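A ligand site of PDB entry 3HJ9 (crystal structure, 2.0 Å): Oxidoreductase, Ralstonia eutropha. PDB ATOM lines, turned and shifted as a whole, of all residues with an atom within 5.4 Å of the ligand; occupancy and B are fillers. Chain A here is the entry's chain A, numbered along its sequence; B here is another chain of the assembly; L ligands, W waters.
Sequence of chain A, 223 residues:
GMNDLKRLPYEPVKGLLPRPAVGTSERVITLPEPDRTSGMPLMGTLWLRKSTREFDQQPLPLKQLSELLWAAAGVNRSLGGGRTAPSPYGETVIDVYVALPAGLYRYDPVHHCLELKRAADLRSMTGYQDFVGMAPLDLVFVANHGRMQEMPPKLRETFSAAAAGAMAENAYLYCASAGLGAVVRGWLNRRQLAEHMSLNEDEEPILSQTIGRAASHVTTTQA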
ATOM      1  N   TYR A  10      -9.874  18.002 -15.039  1.00  0.00           N
ATOM      2  CA  TYR A  10      -8.998  18.589 -14.022  1.00  0.00           C
ATOM      3  C   TYR A  10      -7.957  17.601 -13.496  1.00  0.00           C
ATOM      4  O   TYR A  10      -8.158  16.384 -13.518  1.00  0.00           O
ATOM      5  CB  TYR A  10      -9.796  19.137 -12.841  1.00  0.00           C
ATOM      6  CG  TYR A  10     -10.758  20.260 -13.200  1.00  0.00           C
ATOM      7  CD1 TYR A  10     -10.293  21.429 -13.830  1.00  0.00           C
ATOM      8  CD2 TYR A  10     -12.100  20.167 -12.901  1.00  0.00           C
ATOM      9  CE1 TYR A  10     -11.169  22.463 -14.153  1.00  0.00           C
ATOM     10  CE2 TYR A  10     -12.997  21.190 -13.215  1.00  0.00           C
ATOM     11  CZ  TYR A  10     -12.520  22.325 -13.849  1.00  0.00           C
ATOM     12  OH  TYR A  10     -13.393  23.308 -14.161  1.00  0.00           O
ATOM     13  N   ARG A  49     -27.580  35.569  -8.989  1.00  0.00           N
ATOM     14  CA  ARG A  49     -27.136  34.159  -8.826  1.00  0.00           C
ATOM     15  C   ARG A  49     -25.919  33.956  -9.746  1.00  0.00           C
ATOM     16  O   ARG A  49     -25.984  34.246 -10.943  1.00  0.00           O
ATOM     17  CB  ARG A  49     -28.298  33.215  -9.129  1.00  0.00           C
ATOM     18  CG  ARG A  49     -28.233  31.785  -8.511  1.00  0.00           C
ATOM     19  CD  ARG A  49     -27.073  30.929  -8.964  1.00  0.00           C
ATOM     20  NE  ARG A  49     -26.895  30.957 -10.418  1.00  0.00           N
ATOM     21  CZ  ARG A  49     -25.792  30.621 -11.082  1.00  0.00           C
ATOM     22  NH1 ARG A  49     -24.709  30.161 -10.457  1.00  0.00           N
ATOM     23  NH2 ARG A  49     -25.764  30.752 -12.406  1.00  0.00           N
ATOM     24  N   LYS A  50     -24.786  33.586  -9.142  1.00  0.00           N
ATOM     25  CA  LYS A  50     -23.503  33.426  -9.849  1.00  0.00           C
ATOM     26  C   LYS A  50     -22.558  32.541  -9.058  1.00  0.00           C
ATOM     27  O   LYS A  50     -22.799  32.307  -7.873  1.00  0.00           O
ATOM     28  CB  LYS A  50     -22.818  34.802 -10.048  1.00  0.00           C
ATOM     29  CG  LYS A  50     -22.361  35.500  -8.729  1.00  0.00           C
ATOM     30  CD  LYS A  50     -21.652  36.822  -8.954  1.00  0.00           C
ATOM     31  CE  LYS A  50     -20.303  36.655  -9.656  1.00  0.00           C
ATOM     32  NZ  LYS A  50     -19.542  37.973  -9.733  1.00  0.00           N
ATOM     33  N   SER A  51     -21.461  32.133  -9.681  1.00  0.00           N
ATOM     34  CA  SER A  51     -20.420  31.349  -9.024  1.00  0.00           C
ATOM     35  C   SER A  51     -19.221  32.212  -8.627  1.00  0.00           C
ATOM     36  O   SER A  51     -18.776  33.058  -9.367  1.00  0.00           O
ATOM     37  CB  SER A  51     -19.993  30.143  -9.865  1.00  0.00           C
ATOM     38  OG  SER A  51     -21.056  29.211  -9.917  1.00  0.00           O
ATOM     39  N   ARG A  53     -15.228  31.903  -6.786  1.00  0.00           N
ATOM     40  CA  ARG A  53     -14.142  30.955  -6.560  1.00  0.00           C
ATOM     41  C   ARG A  53     -13.004  31.413  -5.654  1.00  0.00           C
ATOM     42  O   ARG A  53     -12.186  30.587  -5.281  1.00  0.00           O
ATOM     43  CB  ARG A  53     -13.589  30.452  -7.910  1.00  0.00           C
ATOM     44  CG  ARG A  53     -14.541  29.530  -8.638  1.00  0.00           C
ATOM     45  CD  ARG A  53     -13.918  28.834  -9.879  1.00  0.00           C
ATOM     46  NE  ARG A  53     -14.973  28.076 -10.578  1.00  0.00           N
ATOM     47  CZ  ARG A  53     -15.908  28.611 -11.387  1.00  0.00           C
ATOM     48  NH1 ARG A  53     -15.954  29.929 -11.604  1.00  0.00           N
ATOM     49  NH2 ARG A  53     -16.836  27.839 -11.965  1.00  0.00           N
ATOM     50  N   ASP A 130      -9.695  22.262  -9.454  1.00  0.00           N
ATOM     51  CA  ASP A 130     -10.636  23.087 -10.229  1.00  0.00           C
ATOM     52  C   ASP A 130     -10.483  24.596  -9.948  1.00  0.00           C
ATOM     53  O   ASP A 130     -11.387  25.372 -10.251  1.00  0.00           O
ATOM     54  CB  ASP A 130     -12.079  22.593 -10.048  1.00  0.00           C
ATOM     55  CG  ASP A 130     -12.577  22.705  -8.613  1.00  0.00           C
ATOM     56  OD1 ASP A 130     -11.816  23.163  -7.756  1.00  0.00           O
ATOM     57  OD2 ASP A 130     -13.744  22.312  -8.326  1.00  0.00           O
ATOM     58  N   VAL A 132     -10.670  26.407  -7.322  1.00  0.00           N
ATOM     59  CA  VAL A 132     -11.579  26.997  -6.327  1.00  0.00           C
ATOM     60  C   VAL A 132     -10.715  27.187  -5.074  1.00  0.00           C
ATOM     61  O   VAL A 132     -10.125  26.236  -4.605  1.00  0.00           O
ATOM     62  CB  VAL A 132     -12.746  26.092  -6.015  1.00  0.00           C
ATOM     63  CG1 VAL A 132     -13.572  26.659  -4.830  1.00  0.00           C
ATOM     64  CG2 VAL A 132     -13.604  25.908  -7.257  1.00  0.00           C
ATOM     65  N   TYR A 172     -27.291  28.648  -3.378  1.00  0.00           N
ATOM     66  CA  TYR A 172     -26.857  29.747  -4.288  1.00  0.00           C
ATOM     67  C   TYR A 172     -27.673  31.022  -4.141  1.00  0.00           C
ATOM     68  O   TYR A 172     -27.114  32.112  -3.999  1.00  0.00           O
ATOM     69  CB  TYR A 172     -26.952  29.334  -5.757  1.00  0.00           C
ATOM     70  CG  TYR A 172     -25.713  28.812  -6.416  1.00  0.00           C
ATOM     71  CD1 TYR A 172     -24.627  29.654  -6.663  1.00  0.00           C
ATOM     72  CD2 TYR A 172     -25.662  27.501  -6.926  1.00  0.00           C
ATOM     73  CE1 TYR A 172     -23.463  29.168  -7.377  1.00  0.00           C
ATOM     74  CE2 TYR A 172     -24.536  27.031  -7.639  1.00  0.00           C
ATOM     75  CZ  TYR A 172     -23.459  27.843  -7.852  1.00  0.00           C
ATOM     76  OH  TYR A 172     -22.396  27.338  -8.562  1.00  0.00           O
ATOM     77  N   VAL A 183     -20.006  28.249  -5.013  1.00  0.00           N
ATOM     78  CA  VAL A 183     -19.701  27.521  -6.278  1.00  0.00           C
ATOM     79  C   VAL A 183     -19.966  26.042  -6.027  1.00  0.00           C
ATOM     80  O   VAL A 183     -19.433  25.477  -5.067  1.00  0.00           O
ATOM     81  CB  VAL A 183     -18.304  27.794  -6.830  1.00  0.00           C
ATOM     82  CG1 VAL A 183     -17.212  27.359  -5.867  1.00  0.00           C
ATOM     83  CG2 VAL A 183     -18.090  27.120  -8.243  1.00  0.00           C
ATOM     84  N   VAL A 184     -20.915  25.468  -6.789  1.00  0.00           N
ATOM     85  CA  VAL A 184     -21.218  24.049  -6.739  1.00  0.00           C
ATOM     86  C   VAL A 184     -20.078  23.348  -7.508  1.00  0.00           C
ATOM     87  O   VAL A 184     -19.527  23.882  -8.500  1.00  0.00           O
ATOM     88  CB  VAL A 184     -22.643  23.704  -7.306  1.00  0.00           C
ATOM     89  CG1 VAL A 184     -22.753  23.967  -8.830  1.00  0.00           C
ATOM     90  CG2 VAL A 184     -22.982  22.248  -6.955  1.00  0.00           C
ATOM     91  N   ARG A 185     -19.643  22.187  -7.007  1.00  0.00           N
ATOM     92  CA  ARG A 185     -18.526  21.419  -7.583  1.00  0.00           C
ATOM     93  C   ARG A 185     -18.935  19.965  -7.673  1.00  0.00           C
ATOM     94  O   ARG A 185     -19.338  19.356  -6.663  1.00  0.00           O
ATOM     95  CB  ARG A 185     -17.250  21.592  -6.779  1.00  0.00           C
ATOM     96  CG  ARG A 185     -16.985  23.036  -6.382  1.00  0.00           C
ATOM     97  CD  ARG A 185     -16.008  23.139  -5.256  1.00  0.00           C
ATOM     98  NE  ARG A 185     -14.654  22.807  -5.610  1.00  0.00           N
ATOM     99  CZ  ARG A 185     -13.638  22.774  -4.745  1.00  0.00           C
ATOM    100  NH1 ARG A 185     -13.823  23.057  -3.463  1.00  0.00           N
ATOM    101  NH2 ARG A 185     -12.430  22.465  -5.152  1.00  0.00           N
ATOM    102  N   GLY A 186     -18.847  19.435  -8.885  1.00  0.00           N
ATOM    103  CA  GLY A 186     -19.206  18.069  -9.224  1.00  0.00           C
ATOM    104  C   GLY A 186     -18.023  17.208  -9.540  1.00  0.00           C
ATOM    105  O   GLY A 186     -18.175  16.010  -9.656  1.00  0.00           O
ATOM    106  N   TRP A 187     -16.858  17.814  -9.746  1.00  0.00           N
ATOM    107  CA  TRP A 187     -15.622  17.084  -9.915  1.00  0.00           C
ATOM    108  C   TRP A 187     -15.181  16.607  -8.544  1.00  0.00           C
ATOM    109  O   TRP A 187     -14.372  17.271  -7.861  1.00  0.00           O
ATOM    110  CB  TRP A 187     -14.550  17.932 -10.572  1.00  0.00           C
ATOM    111  CG  TRP A 187     -14.647  17.918 -12.040  1.00  0.00           C
ATOM    112  CD1 TRP A 187     -15.396  18.729 -12.830  1.00  0.00           C
ATOM    113  CD2 TRP A 187     -13.966  17.005 -12.901  1.00  0.00           C
ATOM    114  NE1 TRP A 187     -15.178  18.409 -14.154  1.00  0.00           N
ATOM    115  CE2 TRP A 187     -14.311  17.354 -14.227  1.00  0.00           C
ATOM    116  CE3 TRP A 187     -13.063  15.961 -12.678  1.00  0.00           C
ATOM    117  CZ2 TRP A 187     -13.819  16.660 -15.322  1.00  0.00           C
ATOM    118  CZ3 TRP A 187     -12.556  15.262 -13.787  1.00  0.00           C
ATOM    119  CH2 TRP A 187     -12.924  15.632 -15.086  1.00  0.00           C
ATOM    120  N   LEU A 207     -22.289  16.082  -4.982  1.00  0.00           N
ATOM    121  CA  LEU A 207     -21.817  17.435  -5.252  1.00  0.00           C
ATOM    122  C   LEU A 207     -21.313  18.045  -3.968  1.00  0.00           C
ATOM    123  O   LEU A 207     -21.749  17.652  -2.879  1.00  0.00           O
ATOM    124  CB  LEU A 207     -22.982  18.327  -5.713  1.00  0.00           C
ATOM    125  CG  LEU A 207     -23.741  18.058  -6.985  1.00  0.00           C
ATOM    126  CD1 LEU A 207     -25.007  18.968  -7.033  1.00  0.00           C
ATOM    127  CD2 LEU A 207     -22.841  18.237  -8.235  1.00  0.00           C
ATOM    128  N   ARG B  77     -26.981  37.823 -16.919  1.00  0.00           N
ATOM    129  CA  ARG B  77     -25.777  38.632 -17.211  1.00  0.00           C
ATOM    130  C   ARG B  77     -25.544  38.739 -18.735  1.00  0.00           C
ATOM    131  O   ARG B  77     -25.037  37.796 -19.360  1.00  0.00           O
ATOM    132  CB  ARG B  77     -24.564  38.046 -16.506  1.00  0.00           C
ATOM    133  CG  ARG B  77     -24.555  38.253 -14.980  1.00  0.00           C
ATOM    134  CD  ARG B  77     -23.721  37.162 -14.303  1.00  0.00           C
ATOM    135  NE  ARG B  77     -24.391  35.854 -14.357  1.00  0.00           N
ATOM    136  CZ  ARG B  77     -23.827  34.681 -14.067  1.00  0.00           C
ATOM    137  NH1 ARG B  77     -22.539  34.599 -13.747  1.00  0.00           N
ATOM    138  NH2 ARG B  77     -24.549  33.572 -14.135  1.00  0.00           N
ATOM    139  N   GLY B  82     -24.308  34.676 -18.906  1.00  0.00           N
ATOM    140  CA  GLY B  82     -24.447  33.948 -17.654  1.00  0.00           C
ATOM    141  C   GLY B  82     -25.919  33.752 -17.347  1.00  0.00           C
ATOM    142  O   GLY B  82     -26.719  34.632 -17.645  1.00  0.00           O
ATOM    143  N   ARG B  83     -26.256  32.586 -16.809  1.00  0.00           N
ATOM    144  CA  ARG B  83     -27.643  32.191 -16.592  1.00  0.00           C
ATOM    145  C   ARG B  83     -28.029  32.265 -15.122  1.00  0.00           C
ATOM    146  O   ARG B  83     -27.166  32.385 -14.230  1.00  0.00           O
ATOM    147  CB  ARG B  83     -27.917  30.789 -17.149  1.00  0.00           C
ATOM    148  CG  ARG B  83     -27.476  30.527 -18.586  1.00  0.00           C
ATOM    149  CD  ARG B  83     -28.252  31.346 -19.597  1.00  0.00           C
ATOM    150  NE  ARG B  83     -27.510  31.507 -20.840  1.00  0.00           N
ATOM    151  CZ  ARG B  83     -27.540  30.701 -21.897  1.00  0.00           C
ATOM    152  NH1 ARG B  83     -28.287  29.593 -21.951  1.00  0.00           N
ATOM    153  NH2 ARG B  83     -26.807  31.003 -22.927  1.00  0.00           N
ATOM    154  N   ALA B  85     -29.247  29.838 -13.517  1.00  0.00           N
ATOM    155  CA  ALA B  85     -28.811  28.576 -12.879  1.00  0.00           C
ATOM    156  C   ALA B  85     -27.387  28.252 -13.314  1.00  0.00           C
ATOM    157  O   ALA B  85     -26.963  28.660 -14.414  1.00  0.00           O
ATOM    158  CB  ALA B  85     -29.737  27.487 -13.250  1.00  0.00           C
ATOM    159  N   PRO B  86     -26.623  27.526 -12.475  1.00  0.00           N
ATOM    160  CA  PRO B  86     -25.279  27.158 -12.874  1.00  0.00           C
ATOM    161  C   PRO B  86     -25.331  26.085 -13.973  1.00  0.00           C
ATOM    162  O   PRO B  86     -26.378  25.424 -14.194  1.00  0.00           O
ATOM    163  CB  PRO B  86     -24.677  26.605 -11.582  1.00  0.00           C
ATOM    164  CG  PRO B  86     -25.854  25.991 -10.893  1.00  0.00           C
ATOM    165  CD  PRO B  86     -26.944  26.971 -11.146  1.00  0.00           C
ATOM    166  N   SER B  87     -24.219  25.949 -14.674  1.00  0.00           N
ATOM    167  CA  SER B  87     -24.080  24.911 -15.717  1.00  0.00           C
ATOM    168  C   SER B  87     -22.618  24.481 -15.838  1.00  0.00           C
ATOM    169  O   SER B  87     -21.724  25.340 -15.749  1.00  0.00           O
ATOM    170  CB  SER B  87     -24.563  25.436 -17.067  1.00  0.00           C
ATOM    171  OG  SER B  87     -23.696  26.497 -17.512  1.00  0.00           O
ATOM    172  N   PRO B  88     -22.362  23.184 -16.093  1.00  0.00           N
ATOM    173  CA  PRO B  88     -20.980  22.728 -16.210  1.00  0.00           C
ATOM    174  C   PRO B  88     -20.221  23.479 -17.287  1.00  0.00           C
ATOM    175  O   PRO B  88     -20.731  23.612 -18.386  1.00  0.00           O
ATOM    176  CB  PRO B  88     -21.143  21.256 -16.546  1.00  0.00           C
ATOM    177  CG  PRO B  88     -22.475  21.176 -17.146  1.00  0.00           C
ATOM    178  CD  PRO B  88     -23.295  22.089 -16.383  1.00  0.00           C
ATOM    179  N   TYR B  89     -19.058  24.038 -16.910  1.00  0.00           N
ATOM    180  CA  TYR B  89     -18.145  24.800 -17.784  1.00  0.00           C
ATOM    181  C   TYR B  89     -18.762  26.098 -18.343  1.00  0.00           C
ATOM    182  O   TYR B  89     -18.224  26.709 -19.247  1.00  0.00           O
ATOM    183  CB  TYR B  89     -17.595  23.917 -18.914  1.00  0.00           C
ATOM    184  CG  TYR B  89     -16.929  22.672 -18.405  1.00  0.00           C
ATOM    185  CD1 TYR B  89     -15.624  22.714 -17.913  1.00  0.00           C
ATOM    186  CD2 TYR B  89     -17.616  21.457 -18.379  1.00  0.00           C
ATOM    187  CE1 TYR B  89     -14.998  21.573 -17.430  1.00  0.00           C
ATOM    188  CE2 TYR B  89     -16.995  20.296 -17.889  1.00  0.00           C
ATOM    189  CZ  TYR B  89     -15.702  20.358 -17.422  1.00  0.00           C
ATOM    190  OH  TYR B  89     -15.090  19.226 -16.936  1.00  0.00           O
ATOM    191  N   GLY B  90     -19.843  26.549 -17.755  1.00  0.00           N
ATOM    192  CA  GLY B  90     -20.604  27.694 -18.222  1.00  0.00           C
ATOM    193  C   GLY B  90     -21.324  27.441 -19.544  1.00  0.00           C
ATOM    194  O   GLY B  90     -21.777  28.379 -20.163  1.00  0.00           O
ATOM    195  N   THR B 158     -24.786  13.036 -14.165  1.00  0.00           N
ATOM    196  CA  THR B 158     -24.764  13.832 -12.923  1.00  0.00           C
ATOM    197  C   THR B 158     -24.864  15.338 -13.218  1.00  0.00           C
ATOM    198  O   THR B 158     -25.661  16.036 -12.619  1.00  0.00           O
ATOM    199  CB  THR B 158     -23.451  13.566 -12.077  1.00  0.00           C
ATOM    200  OG1 THR B 158     -23.358  12.175 -11.731  1.00  0.00           O
ATOM    201  CG2 THR B 158     -23.433  14.394 -10.770  1.00  0.00           C
ATOM    202  N   PHE B 159     -24.066  15.817 -14.174  1.00  0.00           N
ATOM    203  CA  PHE B 159     -23.995  17.251 -14.501  1.00  0.00           C
ATOM    204  C   PHE B 159     -25.273  17.785 -15.127  1.00  0.00           C
ATOM    205  O   PHE B 159     -25.756  18.827 -14.744  1.00  0.00           O
ATOM    206  CB  PHE B 159     -22.759  17.568 -15.351  1.00  0.00           C
ATOM    207  CG  PHE B 159     -21.441  17.598 -14.574  1.00  0.00           C
ATOM    208  CD1 PHE B 159     -21.281  16.992 -13.297  1.00  0.00           C
ATOM    209  CD2 PHE B 159     -20.316  18.116 -15.183  1.00  0.00           C
ATOM    210  CE1 PHE B 159     -20.050  17.012 -12.640  1.00  0.00           C
ATOM    211  CE2 PHE B 159     -19.066  18.128 -14.550  1.00  0.00           C
ATOM    212  CZ  PHE B 159     -18.943  17.590 -13.259  1.00  0.00           C
ATOM    213  N   ALA B 162     -28.024  17.587 -12.327  1.00  0.00           N
ATOM    214  CA  ALA B 162     -27.828  18.644 -11.317  1.00  0.00           C
ATOM    215  C   ALA B 162     -28.196  20.046 -11.886  1.00  0.00           C
ATOM    216  O   ALA B 162     -28.825  20.851 -11.190  1.00  0.00           O
ATOM    217  CB  ALA B 162     -26.400  18.642 -10.738  1.00  0.00           C
ATOM    218  N   ALA B 163     -27.850  20.290 -13.163  1.00  0.00           N
ATOM    219  CA  ALA B 163     -28.218  21.541 -13.850  1.00  0.00           C
ATOM    220  C   ALA B 163     -29.738  21.611 -13.987  1.00  0.00           C
ATOM    221  O   ALA B 163     -30.339  22.657 -13.660  1.00  0.00           O
ATOM    222  CB  ALA B 163     -27.518  21.654 -15.261  1.00  0.00           C
HETATM  223  N1  LIG L   1     -17.232  24.741 -10.961  1.00  0.00           N
HETATM  224  C1  LIG L   1     -15.962  24.376 -10.538  1.00  0.00           C
HETATM  225  O1  LIG L   1     -15.100  25.240 -10.359  1.00  0.00           O
HETATM  226  N2  LIG L   1     -15.690  23.033 -10.283  1.00  0.00           N
HETATM  227  C2  LIG L   1     -16.646  22.053 -10.494  1.00  0.00           C
HETATM  228  O2  LIG L   1     -16.350  20.878 -10.256  1.00  0.00           O
HETATM  229  C3  LIG L   1     -17.934  22.417 -10.935  1.00  0.00           C
HETATM  230  N3  LIG L   1     -18.911  21.468 -11.143  1.00  0.00           N
HETATM  231  C4  LIG L   1     -20.197  21.837 -11.506  1.00  0.00           C
HETATM  232  C5  LIG L   1     -21.136  20.831 -11.664  1.00  0.00           C
HETATM  233  C6  LIG L   1     -22.446  21.160 -12.052  1.00  0.00           C
HETATM  234  C7  LIG L   1     -23.469  20.060 -12.224  1.00  0.00           C
HETATM  235  C8  LIG L   1     -22.801  22.490 -12.297  1.00  0.00           C
HETATM  236  C9  LIG L   1     -24.200  22.831 -12.736  1.00  0.00           C
HETATM  237  C10 LIG L   1     -21.840  23.503 -12.157  1.00  0.00           C
HETATM  238  C11 LIG L   1     -20.526  23.190 -11.762  1.00  0.00           C
HETATM  239  N4  LIG L   1     -19.525  24.146 -11.571  1.00  0.00           N
HETATM  240  C12 LIG L   1     -18.223  23.773 -11.178  1.00  0.00           C
HETATM  241  C13 LIG L   1     -19.786  25.621 -11.729  1.00  0.00           C
HETATM  242  C14 LIG L   1     -19.743  26.104 -13.152  1.00  0.00           C
HETATM  243  O3  LIG L   1     -18.412  26.135 -13.636  1.00  0.00           O
HETATM  244  C15 LIG L   1     -20.374  27.498 -13.183  1.00  0.00           C
HETATM  245  O4  LIG L   1     -21.760  27.338 -12.928  1.00  0.00           O
HETATM  246  C16 LIG L   1     -20.123  28.138 -14.562  1.00  0.00           C
HETATM  247  O5  LIG L   1     -18.783  28.629 -14.527  1.00  0.00           O
HETATM  248  C17 LIG L   1     -21.089  29.260 -14.899  1.00  0.00           C
HETATM  249  O6  LIG L   1     -20.883  30.291 -13.943  1.00  0.00           O
HETATM  250  P1  LIG L   1     -22.112  30.838 -13.083  1.00  0.00           P
HETATM  251  O7  LIG L   1     -23.355  31.066 -13.898  1.00  0.00           O
HETATM  252  O8  LIG L   1     -22.429  29.797 -12.016  1.00  0.00           O
HETATM  253  O9  LIG L   1     -21.664  32.146 -12.444  1.00  0.00           O
HETATM  254  O   HOH W   1     -24.243  30.803 -16.384  1.00  0.00           O
HETATM  255  O   HOH W   2     -16.344  27.506 -15.287  1.00  0.00           O
HETATM  256  O   HOH W   3     -12.516  26.092 -12.433  1.00  0.00           O
HETATM  257  O   HOH W   4     -17.783  30.863 -13.437  1.00  0.00           O
HETATM  258  O   HOH W   5     -15.299  25.684 -13.375  1.00  0.00           O
HETATM  259  O   HOH W   6     -19.166  33.052 -12.180  1.00  0.00           O
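The backbone NH of Ser 87 of chain B lies within hydrogen-bond range of an oxygen (O4) of the ligand. N of Ser 51 sits at hydrogen-bond distance from O9 of the ligand (2.8 Å). N of Gly 186 sits at hydrogen-bond distance from N3 of the ligand (3.0 Å). N of Trp 187 lies within hydrogen-bond range of O2 of the ligand (3.1 Å). An oxygen (O8) of the ligand is in hydrogen-bond range of the side-chain hydroxyl (OG) of Ser 51 (2.6 Å). The guanidinium group of Arg 53 lies within hydrogen-bond range of an oxygen (O1) of the ligand, at 2.8 Å. An oxygen (O4) of the ligand lies close to the backbone carbonyl oxygen (O) of Ser 87 of chain B, 3.5 Å away. An oxygen (O7) of the ligand is in salt-bridge range of the guanidinium group of Arg 77 of chain B (2.8 Å). The side-chain carboxylate (OD2) of Asp 130 is in hydrogen-bond range of a nitrogen (N2) of the ligand, at 2.9 Å. The guanidinium group (NH1) of Arg 49 is in salt-bridge range of an oxygen (O8) of the ligand (2.8 Å).
The backbone carbonyl oxygen (O) of Arg 77 of chain B sits at hydrogen-bond distance from the backbone NH (N) of Gly 82 of chain B, at 3.2 Å. The guanidinium group (NH2) of Arg 49 sits close to the backbone carbonyl oxygen (O) of Ala 85 of chain B (3.1 Å). The side-chain carboxylate (OD1) of Asp 130 lies close to the backbone NH (N) of Val 132 (3.5 Å). The backbone carbonyl oxygen (O) of Arg 83 of chain B lies within hydrogen-bond range of the guanidinium group (NH2) of Arg 77 of chain B, 2.9 Å away. The side-chain carboxylate (OD1) of Asp 130 is in salt-bridge range of the guanidinium group (NH2) of Arg 185 (2.8 Å). NH2 of Arg 49 is in hydrogen-bond range of O of Arg 83 of chain B (2.8 Å). The side-chain hydroxyl (OH) of Tyr 172 sits at hydrogen-bond distance from the side-chain hydroxyl (OG) of Ser 51, at 2.7 Å. OH of Tyr 172 is in hydrogen-bond range of N of Val 184.
The backbone carbonyl oxygen (O) of Val 184 lies close to a nitrogen (N4) of the ligand (3.1 Å). Residues that only touch the ligand: Lys 50 (3.4 Å), Val 132 (3.5 Å), Val 183 (3.7 Å), Arg 185 (3.5 Å), Pro 86 of chain B (3.3 Å), Pro 88 of chain B (3.8 Å), Tyr 89 of chain B (3.9 Å), Gly 90 of chain B (3.6 Å), Phe 159 of chain B (3.6 Å) and Ala 162 of chain B (3.6 Å). Hydrophobic or aromatic side chains that line the ligand: Val 132, Val 183, Val 184, Trp 187, Pro 86 of chain B, Pro 88 of chain B, Phe 159 of chain B and Ala 162 of chain B. Within 4 Å of the ligand: Arg 49, Lys 50, Ser 51, Arg 53, Asp 130, Val 132, Val 183, Val 184, Arg 185, Gly 186, Trp 187, Arg 77 of chain B, Pro 86 of chain B, Ser 87 of chain B, Pro 88 of chain B, Tyr 89 of chain B, Gly 90 of chain B, Phe 159 of chain B and Ala 162 of chain B. The nearest printed residue that does not touch the ligand is Arg 83 of chain B (4.05 Å).
Water W1 lies within hydrogen-bond range of O7 of the ligand (2.7 Å) and N of Arg 83 of chain B (2.7 Å). Water W6 lies within hydrogen-bond range of an oxygen (O9) of the ligand (2.7 Å) and the backbone carbonyl oxygen (O) of Ser 51 (2.8 Å). Water W4 lies within hydrogen-bond range of an oxygen (O5) of the ligand (2.7 Å) and the guanidinium group of Arg 53 (2.8 Å). Water W2 bridges an oxygen (O5) of the ligand (2.8 Å) and the guanidinium group (NH2) of Arg 53 (3.4 Å). Water W5 lies within hydrogen-bond range of the guanidinium group of Arg 53 (3.0 Å), an oxygen (O1) of the ligand (3.1 Å) and the side-chain hydroxyl of Tyr 10 (3.1 Å). Water W3 lies within hydrogen-bond range of the backbone carbonyl oxygen (O) of Asp 130, the side-chain hydroxyl (OH) of Tyr 10 and an oxygen (O1) of the ligand.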
